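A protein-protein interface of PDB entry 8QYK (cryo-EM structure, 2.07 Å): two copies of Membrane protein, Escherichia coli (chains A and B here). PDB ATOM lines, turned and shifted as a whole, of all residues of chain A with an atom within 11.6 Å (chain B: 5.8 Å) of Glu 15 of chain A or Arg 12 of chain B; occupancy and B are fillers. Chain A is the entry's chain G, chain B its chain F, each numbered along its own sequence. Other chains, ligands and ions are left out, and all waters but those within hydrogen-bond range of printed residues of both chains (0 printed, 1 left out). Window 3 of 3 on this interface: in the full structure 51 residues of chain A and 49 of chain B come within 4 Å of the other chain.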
ATOM      1  N   LYS A   9     -37.947  19.828  27.588  1.00  0.00           N
ATOM      2  CA  LYS A   9     -36.893  20.630  26.918  1.00  0.00           C
ATOM      3  C   LYS A   9     -35.956  21.232  27.960  1.00  0.00           C
ATOM      4  O   LYS A   9     -36.414  22.069  28.721  1.00  0.00           O
ATOM      5  CB  LYS A   9     -37.471  21.756  26.072  1.00  0.00           C
ATOM      6  CG  LYS A   9     -37.341  21.570  24.569  1.00  0.00           C
ATOM      7  CD  LYS A   9     -38.074  20.354  24.047  1.00  0.00           C
ATOM      8  CE  LYS A   9     -39.574  20.444  24.216  1.00  0.00           C
ATOM      9  NZ  LYS A   9     -40.279  19.396  23.439  1.00  0.00           N
ATOM     10  N   LYS A  10     -34.690  20.834  27.918  1.00  0.00           N
ATOM     11  CA  LYS A  10     -33.728  21.320  28.922  1.00  0.00           C
ATOM     12  C   LYS A  10     -33.753  22.843  28.909  1.00  0.00           C
ATOM     13  O   LYS A  10     -33.775  23.405  27.808  1.00  0.00           O
ATOM     14  CB  LYS A  10     -32.333  20.759  28.626  1.00  0.00           C
ATOM     15  CG  LYS A  10     -32.095  19.308  29.001  1.00  0.00           C
ATOM     16  CD  LYS A  10     -30.661  19.055  29.366  1.00  0.00           C
ATOM     17  CE  LYS A  10     -30.343  19.497  30.776  1.00  0.00           C
ATOM     18  NZ  LYS A  10     -29.032  18.969  31.214  1.00  0.00           N
ATOM     19  N   ARG A  11     -33.755  23.473  30.092  1.00  0.00           N
ATOM     20  CA  ARG A  11     -33.694  24.951  30.240  1.00  0.00           C
ATOM     21  C   ARG A  11     -32.467  25.576  29.557  1.00  0.00           C
ATOM     22  O   ARG A  11     -31.453  24.897  29.426  1.00  0.00           O
ATOM     23  CB  ARG A  11     -33.686  25.298  31.733  1.00  0.00           C
ATOM     24  CG  ARG A  11     -32.448  25.988  32.284  1.00  0.00           C
ATOM     25  CD  ARG A  11     -32.119  25.545  33.696  1.00  0.00           C
ATOM     26  NE  ARG A  11     -33.253  25.000  34.433  1.00  0.00           N
ATOM     27  CZ  ARG A  11     -33.161  24.114  35.420  1.00  0.00           C
ATOM     28  NH1 ARG A  11     -34.254  23.651  35.996  1.00  0.00           N
ATOM     29  NH2 ARG A  11     -31.979  23.690  35.836  1.00  0.00           N
ATOM     30  N   ARG A  12     -32.578  26.834  29.133  1.00  0.00           N
ATOM     31  CA  ARG A  12     -31.462  27.609  28.549  1.00  0.00           C
ATOM     32  C   ARG A  12     -30.527  27.864  29.731  1.00  0.00           C
ATOM     33  O   ARG A  12     -30.923  28.565  30.680  1.00  0.00           O
ATOM     34  CB  ARG A  12     -32.106  28.826  27.872  1.00  0.00           C
ATOM     35  CG  ARG A  12     -32.977  28.531  26.657  1.00  0.00           C
ATOM     36  CD  ARG A  12     -33.638  29.746  26.035  1.00  0.00           C
ATOM     37  NE  ARG A  12     -34.447  29.443  24.862  1.00  0.00           N
ATOM     38  CZ  ARG A  12     -35.700  29.011  24.911  1.00  0.00           C
ATOM     39  NH1 ARG A  12     -36.525  29.490  25.826  1.00  0.00           N
ATOM     40  NH2 ARG A  12     -36.118  28.097  24.052  1.00  0.00           N
ATOM     41  N   SER A  13     -29.377  27.220  29.743  1.00  0.00           N
ATOM     42  CA  SER A  13     -28.474  27.282  30.920  1.00  0.00           C
ATOM     43  C   SER A  13     -27.443  28.384  30.744  1.00  0.00           C
ATOM     44  O   SER A  13     -26.529  28.199  29.919  1.00  0.00           O
ATOM     45  CB  SER A  13     -27.854  25.945  31.189  1.00  0.00           C
ATOM     46  OG  SER A  13     -26.960  26.034  32.286  1.00  0.00           O
ATOM     47  N   ASP A  14     -27.599  29.484  31.479  1.00  0.00           N
ATOM     48  CA  ASP A  14     -26.572  30.550  31.469  1.00  0.00           C
ATOM     49  C   ASP A  14     -25.206  29.879  31.496  1.00  0.00           C
ATOM     50  O   ASP A  14     -24.972  28.973  32.316  1.00  0.00           O
ATOM     51  CB  ASP A  14     -26.600  31.474  32.689  1.00  0.00           C
ATOM     52  CG  ASP A  14     -25.549  32.575  32.605  1.00  0.00           C
ATOM     53  OD1 ASP A  14     -25.045  33.005  33.655  1.00  0.00           O
ATOM     54  OD2 ASP A  14     -25.236  32.998  31.480  1.00  0.00           O
ATOM     55  N   GLU A  15     -24.333  30.352  30.637  1.00  0.00           N
ATOM     56  CA  GLU A  15     -23.002  29.741  30.611  1.00  0.00           C
ATOM     57  C   GLU A  15     -22.116  30.605  31.505  1.00  0.00           C
ATOM     58  O   GLU A  15     -22.281  31.818  31.506  1.00  0.00           O
ATOM     59  CB  GLU A  15     -22.570  29.456  29.170  1.00  0.00           C
ATOM     60  CG  GLU A  15     -23.420  28.379  28.514  1.00  0.00           C
ATOM     61  CD  GLU A  15     -23.106  28.080  27.054  1.00  0.00           C
ATOM     62  OE1 GLU A  15     -22.327  28.848  26.454  1.00  0.00           O
ATOM     63  OE2 GLU A  15     -23.621  27.073  26.517  1.00  0.00           O
ATOM     64  N   ALA A  16     -21.235  29.974  32.253  1.00  0.00           N
ATOM     65  CA  ALA A  16     -20.385  30.660  33.234  1.00  0.00           C
ATOM     66  C   ALA A  16     -19.252  31.483  32.649  1.00  0.00           C
ATOM     67  O   ALA A  16     -18.913  31.303  31.506  1.00  0.00           O
ATOM     68  CB  ALA A  16     -19.814  29.582  34.125  1.00  0.00           C
ATOM     69  N   GLU A  17     -18.625  32.239  33.517  1.00  0.00           N
ATOM     70  CA  GLU A  17     -17.435  33.016  33.114  1.00  0.00           C
ATOM     71  C   GLU A  17     -16.338  32.011  32.787  1.00  0.00           C
ATOM     72  O   GLU A  17     -16.057  31.159  33.630  1.00  0.00           O
ATOM     73  CB  GLU A  17     -17.122  34.013  34.227  1.00  0.00           C
ATOM     74  CG  GLU A  17     -15.889  34.863  33.994  1.00  0.00           C
ATOM     75  CD  GLU A  17     -15.859  35.696  32.724  1.00  0.00           C
ATOM     76  OE1 GLU A  17     -16.595  36.695  32.661  1.00  0.00           O
ATOM     77  OE2 GLU A  17     -15.083  35.352  31.810  1.00  0.00           O
ATOM     78  N   LYS A  18     -15.803  32.067  31.572  1.00  0.00           N
ATOM     79  CA  LYS A  18     -14.655  31.247  31.201  1.00  0.00           C
ATOM     80  C   LYS A  18     -13.564  31.416  32.247  1.00  0.00           C
ATOM     81  O   LYS A  18     -13.242  32.554  32.609  1.00  0.00           O
ATOM     82  CB  LYS A  18     -14.132  31.622  29.821  1.00  0.00           C
ATOM     83  CG  LYS A  18     -15.162  31.519  28.723  1.00  0.00           C
ATOM     84  CD  LYS A  18     -14.544  31.807  27.371  1.00  0.00           C
ATOM     85  CE  LYS A  18     -13.490  30.778  27.017  1.00  0.00           C
ATOM     86  NZ  LYS A  18     -12.907  30.990  25.665  1.00  0.00           N
ATOM     87  N   PRO A  19     -13.006  30.331  32.783  1.00  0.00           N
ATOM     88  CA  PRO A  19     -11.974  30.474  33.821  1.00  0.00           C
ATOM     89  C   PRO A  19     -10.745  31.224  33.356  1.00  0.00           C
ATOM     90  O   PRO A  19     -10.069  31.855  34.184  1.00  0.00           O
ATOM     91  CB  PRO A  19     -11.636  29.022  34.179  1.00  0.00           C
ATOM     92  CG  PRO A  19     -12.015  28.235  32.958  1.00  0.00           C
ATOM     93  CD  PRO A  19     -13.215  28.928  32.390  1.00  0.00           C
ATOM     94  N   TRP A  21     -10.247  33.946  31.582  1.00  0.00           N
ATOM     95  CA  TRP A  21     -10.189  35.400  31.645  1.00  0.00           C
ATOM     96  C   TRP A  21     -10.022  35.889  33.077  1.00  0.00           C
ATOM     97  O   TRP A  21      -9.241  36.810  33.332  1.00  0.00           O
ATOM     98  CB  TRP A  21     -11.416  36.008  30.971  1.00  0.00           C
ATOM     99  CG  TRP A  21     -11.340  35.905  29.478  1.00  0.00           C
ATOM    100  CD1 TRP A  21     -12.163  35.189  28.658  1.00  0.00           C
ATOM    101  CD2 TRP A  21     -10.363  36.519  28.626  1.00  0.00           C
ATOM    102  NE1 TRP A  21     -11.769  35.333  27.350  1.00  0.00           N
ATOM    103  CE2 TRP A  21     -10.666  36.143  27.304  1.00  0.00           C
ATOM    104  CE3 TRP A  21      -9.268  37.358  28.855  1.00  0.00           C
ATOM    105  CZ2 TRP A  21      -9.915  36.576  26.216  1.00  0.00           C
ATOM    106  CZ3 TRP A  21      -8.522  37.782  27.774  1.00  0.00           C
ATOM    107  CH2 TRP A  21      -8.849  37.393  26.472  1.00  0.00           C
ATOM    108  N   LYS B  10     -33.910  22.802  17.808  1.00  0.00           N
ATOM    109  CA  LYS B  10     -32.793  23.737  17.940  1.00  0.00           C
ATOM    110  C   LYS B  10     -33.282  25.112  18.410  1.00  0.00           C
ATOM    111  O   LYS B  10     -32.840  26.157  17.933  1.00  0.00           O
ATOM    112  CB  LYS B  10     -31.998  23.812  16.626  1.00  0.00           C
ATOM    113  CG  LYS B  10     -30.710  24.632  16.640  1.00  0.00           C
ATOM    114  CD  LYS B  10     -30.860  25.856  15.746  1.00  0.00           C
ATOM    115  CE  LYS B  10     -29.844  26.926  16.079  1.00  0.00           C
ATOM    116  NZ  LYS B  10     -30.041  28.119  15.216  1.00  0.00           N
ATOM    117  N   ARG B  11     -34.227  25.122  19.344  1.00  0.00           N
ATOM    118  CA  ARG B  11     -34.671  26.376  19.936  1.00  0.00           C
ATOM    119  C   ARG B  11     -33.683  26.791  21.018  1.00  0.00           C
ATOM    120  O   ARG B  11     -33.968  26.667  22.215  1.00  0.00           O
ATOM    121  CB  ARG B  11     -36.091  26.231  20.490  1.00  0.00           C
ATOM    122  CG  ARG B  11     -36.725  27.522  20.979  1.00  0.00           C
ATOM    123  CD  ARG B  11     -38.077  27.238  21.600  1.00  0.00           C
ATOM    124  NE  ARG B  11     -38.974  26.608  20.638  1.00  0.00           N
ATOM    125  CZ  ARG B  11     -39.939  25.757  20.957  1.00  0.00           C
ATOM    126  NH1 ARG B  11     -40.164  25.404  22.212  1.00  0.00           N
ATOM    127  NH2 ARG B  11     -40.698  25.244  19.990  1.00  0.00           N
ATOM    128  N   ARG B  12     -32.507  27.270  20.604  1.00  0.00           N
ATOM    129  CA  ARG B  12     -31.435  27.603  21.541  1.00  0.00           C
ATOM    130  C   ARG B  12     -30.564  28.679  20.897  1.00  0.00           C
ATOM    131  O   ARG B  12     -29.700  28.367  20.072  1.00  0.00           O
ATOM    132  CB  ARG B  12     -30.625  26.363  21.899  1.00  0.00           C
ATOM    133  CG  ARG B  12     -29.619  26.551  23.027  1.00  0.00           C
ATOM    134  CD  ARG B  12     -28.230  26.860  22.492  1.00  0.00           C
ATOM    135  NE  ARG B  12     -27.239  26.949  23.556  1.00  0.00           N
ATOM    136  CZ  ARG B  12     -26.000  27.392  23.390  1.00  0.00           C
ATOM    137  NH1 ARG B  12     -25.566  27.800  22.210  1.00  0.00           N
ATOM    138  NH2 ARG B  12     -25.177  27.425  24.433  1.00  0.00           N
ATOM    139  N   SER B  13     -30.794  29.932  21.278  1.00  0.00           N
ATOM    140  CA  SER B  13     -29.953  31.022  20.802  1.00  0.00           C
ATOM    141  C   SER B  13     -28.623  31.012  21.545  1.00  0.00           C
ATOM    142  O   SER B  13     -28.570  30.705  22.739  1.00  0.00           O
ATOM    143  CB  SER B  13     -30.658  32.363  20.989  1.00  0.00           C
ATOM    144  OG  SER B  13     -30.934  32.609  22.357  1.00  0.00           O
ATOM    145  N   ASP B  14     -27.549  31.346  20.838  1.00  0.00           N
ATOM    146  CA  ASP B  14     -26.227  31.330  21.446  1.00  0.00           C
ATOM    147  C   ASP B  14     -26.066  32.482  22.429  1.00  0.00           C
ATOM    148  O   ASP B  14     -26.363  33.638  22.117  1.00  0.00           O
ATOM    149  CB  ASP B  14     -25.149  31.406  20.366  1.00  0.00           C
ATOM    150  CG  ASP B  14     -25.162  30.203  19.451  1.00  0.00           C
ATOM    151  OD1 ASP B  14     -26.008  30.159  18.534  1.00  0.00           O
ATOM    152  OD2 ASP B  14     -24.328  29.295  19.653  1.00  0.00           O
ATOM    153  N   GLU B  15     -25.592  32.156  23.626  1.00  0.00           N
ATOM    154  CA  GLU B  15     -25.281  33.167  24.625  1.00  0.00           C
ATOM    155  C   GLU B  15     -24.066  33.975  24.195  1.00  0.00           C
ATOM    156  O   GLU B  15     -23.105  33.435  23.640  1.00  0.00           O
ATOM    157  CB  GLU B  15     -25.026  32.511  25.984  1.00  0.00           C
ATOM    158  CG  GLU B  15     -24.027  31.361  25.941  1.00  0.00           C
ATOM    159  CD  GLU B  15     -22.596  31.806  26.185  1.00  0.00           C
ATOM    160  OE1 GLU B  15     -22.398  32.859  26.827  1.00  0.00           O
ATOM    161  OE2 GLU B  15     -21.668  31.104  25.732  1.00  0.00           O
ATOM    162  N   LYS B  18     -19.271  36.840  27.832  1.00  0.00           N
ATOM    163  CA  LYS B  18     -19.193  37.867  28.863  1.00  0.00           C
ATOM    164  C   LYS B  18     -17.934  38.694  28.643  1.00  0.00           C
ATOM    165  O   LYS B  18     -16.830  38.141  28.674  1.00  0.00           O
ATOM    166  CB  LYS B  18     -19.174  37.236  30.245  1.00  0.00           C
ATOM    167  CG  LYS B  18     -20.414  36.436  30.594  1.00  0.00           C
ATOM    168  CD  LYS B  18     -21.556  37.334  31.020  1.00  0.00           C
ATOM    169  CE  LYS B  18     -22.822  36.531  31.268  1.00  0.00           C
ATOM    170  NZ  LYS B  18     -22.648  35.563  32.381  1.00  0.00           N
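Among the printed residues, pairs that only touch across the chains: Glu 17 of chain A with Lys 18 of chain B and Glu 15 of chain A with Lys 18 of chain B.
Arg 12 of chain A touches Arg 11 of chain B, but with the chains exchanged Arg 11 of chain A does not touch Arg 12 of chain B (6.9 Å).
Asp 14 of chain A touches Lys 18 of chain B, but with the chains exchanged Lys 18 of chain A does not touch Asp 14 of chain B (12.6 Å).
Glu 15 of chain A touches Arg 12 of chain B, but with the chains exchanged Arg 12 of chain A does not touch Glu 15 of chain B (8.1 Å).
Glu 15 of chain A touches its own counterpart, Glu 15 of chain B.
Of the 6 pairs that touch across the chains among the printed residues, 1 has its exchanged pair printed and touching as well.
The guanidinium group (NH1) of Arg 12 of chain B lies within salt-bridge range of the side-chain carboxylate (OD2) of Asp 14 of chain B.
The guanidinium group (NH2) of Arg 12 of chain A sits at hydrogen-bond distance from the backbone carbonyl oxygen (O) of Arg 11 of chain B (3.2 Å).
The guanidinium group (NH2) of Arg 12 of chain B lies within salt-bridge range of the side-chain carboxylate (OE2) of Glu 15 of chain A (2.6 Å).
OE2 of Glu 15 of chain B lies close to OE1 of Glu 15 of chain A (2.5 Å).
The side-chain amino group (NZ) of Lys 18 of chain B lies within salt-bridge range of the side-chain carboxylate (OD1) of Asp 14 of chain A (3.7 Å).
Of the 7 printed residues of chain B, 4 touch a printed residue of chain A.
Printed residues of chain B that touch a printed residue of chain A: Arg 11, Arg 12, Glu 15 and Lys 18.
Among the printed residues, 6 pairs touch across the chains.
Among the printed residues, Asp or Glu carboxylates within 4 Å of a Lys or Arg side-chain nitrogen of the other chain: Asp 14 of chain A with Lys 18 of chain B and Glu 15 of chain A with Arg 12 of chain B.
Lys 10 of chain A touches none of the printed residues of chain B.
Of the printed residues of chain B, Asp 14 of chain A touches Lys 18.
Of chain B, only Arg 12, Glu 15 and Lys 18 come within 4 Å of Glu 15 of chain A.
Printed residues of chain B within 4 Å of Glu 17 of chain A: Lys 18.
Of the printed residues of chain A, Arg 11 of chain B touches Arg 12.
Of chain A, only Glu 15 comes within 4 Å of Arg 12 of chain B.
Ser 13 of chain B touches none of the printed residues of chain A.
No residue of chain A comes within 4 Å of Asp 14 of chain B.
Glu 15 of chain B touches one residue of chain A.
The nearest residue of chain A that does not touch Arg 12 of chain B is Arg 12 of chain A (4.8 Å).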
